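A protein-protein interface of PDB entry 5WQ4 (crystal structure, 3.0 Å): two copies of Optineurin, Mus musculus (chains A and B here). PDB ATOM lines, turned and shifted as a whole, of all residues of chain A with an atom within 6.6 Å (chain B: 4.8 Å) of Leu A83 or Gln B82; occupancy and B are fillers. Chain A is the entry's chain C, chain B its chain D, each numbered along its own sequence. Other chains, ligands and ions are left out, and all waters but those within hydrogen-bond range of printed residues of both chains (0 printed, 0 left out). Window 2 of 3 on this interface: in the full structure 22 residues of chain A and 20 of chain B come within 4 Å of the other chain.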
ATOM      1  N   GLN A  78      13.804  28.341   8.999  1.00  0.00           N
ATOM      2  CA  GLN A  78      13.669  29.688   9.535  1.00  0.00           C
ATOM      3  C   GLN A  78      13.768  29.677  11.053  1.00  0.00           C
ATOM      4  O   GLN A  78      14.629  30.344  11.654  1.00  0.00           O
ATOM      5  CB  GLN A  78      12.338  30.313   9.107  1.00  0.00           C
ATOM      6  N   LEU A  79      12.898  28.869  11.655  1.00  0.00           N
ATOM      7  CA  LEU A  79      12.761  28.777  13.104  1.00  0.00           C
ATOM      8  C   LEU A  79      14.099  28.447  13.726  1.00  0.00           C
ATOM      9  O   LEU A  79      14.519  29.078  14.687  1.00  0.00           O
ATOM     10  CB  LEU A  79      11.705  27.703  13.464  1.00  0.00           C
ATOM     11  CG  LEU A  79      10.246  28.128  13.685  1.00  0.00           C
ATOM     12  CD1 LEU A  79       9.944  29.314  12.788  1.00  0.00           C
ATOM     13  CD2 LEU A  79       9.300  26.997  13.357  1.00  0.00           C
ATOM     14  N   ALA A  80      14.799  27.507  13.122  1.00  0.00           N
ATOM     15  CA  ALA A  80      16.109  27.099  13.592  1.00  0.00           C
ATOM     16  C   ALA A  80      17.149  28.230  13.491  1.00  0.00           C
ATOM     17  O   ALA A  80      18.022  28.358  14.354  1.00  0.00           O
ATOM     18  CB  ALA A  80      16.571  25.881  12.827  1.00  0.00           C
ATOM     19  N   LEU A  81      17.101  29.014  12.414  1.00  0.00           N
ATOM     20  CA  LEU A  81      18.026  30.135  12.305  1.00  0.00           C
ATOM     21  C   LEU A  81      17.830  31.004  13.532  1.00  0.00           C
ATOM     22  O   LEU A  81      18.777  31.211  14.318  1.00  0.00           O
ATOM     23  CB  LEU A  81      17.798  30.939  11.022  1.00  0.00           C
ATOM     24  N   GLN A  82      16.595  31.465  13.728  1.00  0.00           N
ATOM     25  CA  GLN A  82      16.305  32.329  14.880  1.00  0.00           C
ATOM     26  C   GLN A  82      16.738  31.658  16.183  1.00  0.00           C
ATOM     27  O   GLN A  82      17.129  32.315  17.144  1.00  0.00           O
ATOM     28  CB  GLN A  82      14.830  32.676  14.959  1.00  0.00           C
ATOM     29  CG  GLN A  82      14.213  33.031  13.649  1.00  0.00           C
ATOM     30  CD  GLN A  82      12.734  33.206  13.796  1.00  0.00           C
ATOM     31  OE1 GLN A  82      12.263  33.709  14.822  1.00  0.00           O
ATOM     32  NE2 GLN A  82      11.977  32.759  12.793  1.00  0.00           N
ATOM     33  N   LEU A  83      16.648  30.338  16.199  1.00  0.00           N
ATOM     34  CA  LEU A  83      17.041  29.559  17.364  1.00  0.00           C
ATOM     35  C   LEU A  83      18.547  29.761  17.636  1.00  0.00           C
ATOM     36  O   LEU A  83      18.933  30.141  18.733  1.00  0.00           O
ATOM     37  CB  LEU A  83      16.684  28.077  17.136  1.00  0.00           C
ATOM     38  CG  LEU A  83      16.343  27.154  18.311  1.00  0.00           C
ATOM     39  CD1 LEU A  83      17.571  26.771  19.131  1.00  0.00           C
ATOM     40  CD2 LEU A  83      15.254  27.817  19.168  1.00  0.00           C
ATOM     41  N   ALA A  84      19.386  29.511  16.636  1.00  0.00           N
ATOM     42  CA  ALA A  84      20.829  29.758  16.740  1.00  0.00           C
ATOM     43  C   ALA A  84      21.208  31.195  17.147  1.00  0.00           C
ATOM     44  O   ALA A  84      21.939  31.395  18.153  1.00  0.00           O
ATOM     45  CB  ALA A  84      21.506  29.407  15.416  1.00  0.00           C
ATOM     46  N   ILE A  85      20.672  32.188  16.417  1.00  0.00           N
ATOM     47  CA  ILE A  85      21.025  33.587  16.697  1.00  0.00           C
ATOM     48  C   ILE A  85      20.569  33.998  18.113  1.00  0.00           C
ATOM     49  O   ILE A  85      21.395  34.452  18.915  1.00  0.00           O
ATOM     50  CB  ILE A  85      20.469  34.607  15.605  1.00  0.00           C
ATOM     51  CG1 ILE A  85      18.939  34.744  15.637  1.00  0.00           C
ATOM     52  CG2 ILE A  85      20.994  34.273  14.169  1.00  0.00           C
ATOM     53  CD1 ILE A  85      18.387  35.832  14.721  1.00  0.00           C
ATOM     54  N   LEU A  86      19.292  33.803  18.450  1.00  0.00           N
ATOM     55  CA  LEU A  86      18.805  34.122  19.802  1.00  0.00           C
ATOM     56  C   LEU A  86      19.538  33.388  20.917  1.00  0.00           C
ATOM     57  O   LEU A  86      19.833  33.990  21.943  1.00  0.00           O
ATOM     58  CB  LEU A  86      17.311  33.819  19.933  1.00  0.00           C
ATOM     59  CG  LEU A  86      16.307  34.920  19.583  1.00  0.00           C
ATOM     60  CD1 LEU A  86      16.259  35.266  18.059  1.00  0.00           C
ATOM     61  CD2 LEU A  86      14.933  34.508  20.124  1.00  0.00           C
ATOM     62  N   LEU A  87      19.845  32.107  20.703  1.00  0.00           N
ATOM     63  CA  LEU A  87      20.523  31.293  21.718  1.00  0.00           C
ATOM     64  C   LEU A  87      21.914  31.802  22.056  1.00  0.00           C
ATOM     65  O   LEU A  87      22.244  31.947  23.237  1.00  0.00           O
ATOM     66  CB  LEU A  87      20.622  29.834  21.285  1.00  0.00           C
ATOM     67  N   LYS A  88      22.750  32.071  21.054  1.00  0.00           N
ATOM     68  CA  LYS A  88      24.078  32.570  21.424  1.00  0.00           C
ATOM     69  C   LYS A  88      24.023  34.059  21.826  1.00  0.00           C
ATOM     70  O   LYS A  88      24.958  34.569  22.450  1.00  0.00           O
ATOM     71  CB  LYS A  88      25.080  32.363  20.288  1.00  0.00           C
ATOM     72  N   GLN B  78       8.545  21.182  17.510  1.00  0.00           N
ATOM     73  CA  GLN B  78       9.504  21.268  18.600  1.00  0.00           C
ATOM     74  C   GLN B  78      10.171  22.612  18.612  1.00  0.00           C
ATOM     75  O   GLN B  78      10.155  23.317  19.630  1.00  0.00           O
ATOM     76  CB  GLN B  78      10.551  20.172  18.504  1.00  0.00           C
ATOM     77  CG  GLN B  78      10.052  18.826  19.050  1.00  0.00           C
ATOM     78  N   LEU B  79      10.773  22.963  17.480  1.00  0.00           N
ATOM     79  CA  LEU B  79      11.437  24.254  17.375  1.00  0.00           C
ATOM     80  C   LEU B  79      10.495  25.416  17.622  1.00  0.00           C
ATOM     81  O   LEU B  79      10.866  26.397  18.260  1.00  0.00           O
ATOM     82  CB  LEU B  79      12.098  24.409  16.018  1.00  0.00           C
ATOM     83  CG  LEU B  79      13.582  24.074  15.921  1.00  0.00           C
ATOM     84  CD1 LEU B  79      13.986  22.934  16.830  1.00  0.00           C
ATOM     85  CD2 LEU B  79      13.871  23.754  14.476  1.00  0.00           C
ATOM     86  N   ALA B  80       9.276  25.314  17.118  1.00  0.00           N
ATOM     87  CA  ALA B  80       8.303  26.379  17.315  1.00  0.00           C
ATOM     88  C   ALA B  80       7.971  26.594  18.793  1.00  0.00           C
ATOM     89  O   ALA B  80       8.042  27.711  19.289  1.00  0.00           O
ATOM     90  CB  ALA B  80       7.046  26.054  16.555  1.00  0.00           C
ATOM     91  N   LEU B  81       7.706  25.501  19.505  1.00  0.00           N
ATOM     92  CA  LEU B  81       7.440  25.539  20.934  1.00  0.00           C
ATOM     93  C   LEU B  81       8.580  26.187  21.646  1.00  0.00           C
ATOM     94  O   LEU B  81       8.409  27.147  22.398  1.00  0.00           O
ATOM     95  CB  LEU B  81       7.268  24.127  21.488  1.00  0.00           C
ATOM     96  CG  LEU B  81       6.538  23.862  22.814  1.00  0.00           C
ATOM     97  CD1 LEU B  81       7.265  22.830  23.570  1.00  0.00           C
ATOM     98  CD2 LEU B  81       6.334  25.082  23.676  1.00  0.00           C
ATOM     99  N   GLN B  82       9.754  25.621  21.421  1.00  0.00           N
ATOM    100  CA  GLN B  82      10.954  26.081  22.092  1.00  0.00           C
ATOM    101  C   GLN B  82      11.211  27.571  21.884  1.00  0.00           C
ATOM    102  O   GLN B  82      11.561  28.286  22.828  1.00  0.00           O
ATOM    103  CB  GLN B  82      12.121  25.241  21.602  1.00  0.00           C
ATOM    104  CG  GLN B  82      13.450  25.885  21.676  1.00  0.00           C
ATOM    105  CD  GLN B  82      14.506  24.926  21.210  1.00  0.00           C
ATOM    106  OE1 GLN B  82      14.186  23.844  20.701  1.00  0.00           O
ATOM    107  NE2 GLN B  82      15.770  25.311  21.359  1.00  0.00           N
ATOM    108  N   LEU B  83      10.954  28.034  20.663  1.00  0.00           N
ATOM    109  CA  LEU B  83      11.097  29.441  20.321  1.00  0.00           C
ATOM    110  C   LEU B  83      10.093  30.309  21.087  1.00  0.00           C
ATOM    111  O   LEU B  83      10.494  31.260  21.746  1.00  0.00           O
ATOM    112  CB  LEU B  83      10.954  29.650  18.814  1.00  0.00           C
ATOM    113  CG  LEU B  83      11.693  30.870  18.231  1.00  0.00           C
ATOM    114  CD1 LEU B  83      10.944  32.198  18.439  1.00  0.00           C
ATOM    115  CD2 LEU B  83      13.103  30.940  18.827  1.00  0.00           C
ATOM    116  N   ALA B  84       8.806  29.957  21.012  1.00  0.00           N
ATOM    117  CA  ALA B  84       7.743  30.638  21.764  1.00  0.00           C
ATOM    118  C   ALA B  84       8.126  30.815  23.243  1.00  0.00           C
ATOM    119  O   ALA B  84       8.000  31.919  23.832  1.00  0.00           O
ATOM    120  CB  ALA B  84       6.433  29.856  21.651  1.00  0.00           C
ATOM    121  N   ILE B  85       8.605  29.720  23.830  1.00  0.00           N
ATOM    122  CA  ILE B  85       9.012  29.728  25.226  1.00  0.00           C
ATOM    123  C   ILE B  85      10.194  30.675  25.499  1.00  0.00           C
ATOM    124  O   ILE B  85      10.112  31.495  26.416  1.00  0.00           O
ATOM    125  CB  ILE B  85       9.320  28.294  25.702  1.00  0.00           C
ATOM    126  CG1 ILE B  85       8.002  27.615  26.079  1.00  0.00           C
ATOM    127  CG2 ILE B  85      10.236  28.293  26.910  1.00  0.00           C
ATOM    128  CD1 ILE B  85       8.118  26.216  26.549  1.00  0.00           C
ATOM    129  N   LEU B  86      11.278  30.559  24.730  1.00  0.00           N
ATOM    130  CA  LEU B  86      12.440  31.465  24.874  1.00  0.00           C
ATOM    131  C   LEU B  86      12.075  32.952  24.710  1.00  0.00           C
ATOM    132  O   LEU B  86      12.585  33.851  25.407  1.00  0.00           O
ATOM    133  CB  LEU B  86      13.512  31.102  23.848  1.00  0.00           C
ATOM    134  CG  LEU B  86      14.894  31.726  24.014  1.00  0.00           C
ATOM    135  CD1 LEU B  86      15.564  31.062  25.186  1.00  0.00           C
ATOM    136  CD2 LEU B  86      15.750  31.616  22.739  1.00  0.00           C
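Leu A79 touches none of the printed residues of chain B.
Of the printed residues of chain B, Ala A80 touches Leu B79.
Printed residues of chain A within 4 Å of Leu B79: Ala A80.
Of chain A, only Leu A83 (3.2 Å) comes within 4 Å of Gln B82.
Printed residues of chain A within 4 Å of Leu B83: Leu A83 (3.8 Å).
Printed residues of chain A within 4 Å of Leu B86: Leu A86 (3.9 Å).
The nearest residue of chain B that does not touch Leu A83 is Leu B79 (4.7 Å).
The nearest printed residue of chain A that does not touch Gln B82 is Leu A87 (6.6 Å).
Among the printed residues, merely in contact across the chains: Leu A83 with Gln B82, Leu A83 with Leu B83, Ala A80 with Leu B79 and Leu A86 with Leu B86.
Ala A80 touches Leu B79, but with the chains exchanged Leu A79 does not touch Ala B80 (4.02 Å).
Leu A83 touches Gln B82, but with the chains exchanged Gln A82 does not touch Leu B83 (4.1 Å).
Leu A83 touches its own counterpart, Leu B83.
Leu A86 touches its own counterpart, Leu B86.
Positions printed for both chains: 78, 79, 80, 81, 82, 83, 84, 85 and 86.
Of the 4 pairs that touch across the chains among the printed residues, 2 have their exchanged pair printed and touching as well.
Of the 9 printed residues of chain B, 4 touch a printed residue of chain A.
Of the 11 printed residues of chain A, 3 touch a printed residue of chain B.
Printed residues of chain A that touch a printed residue of chain B: Ala A80, Leu A83 and Leu A86.
Hydrophobic or aromatic side chains of chain A that line the printed part of chain B: Ala A80, Leu A83 and Leu A86.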
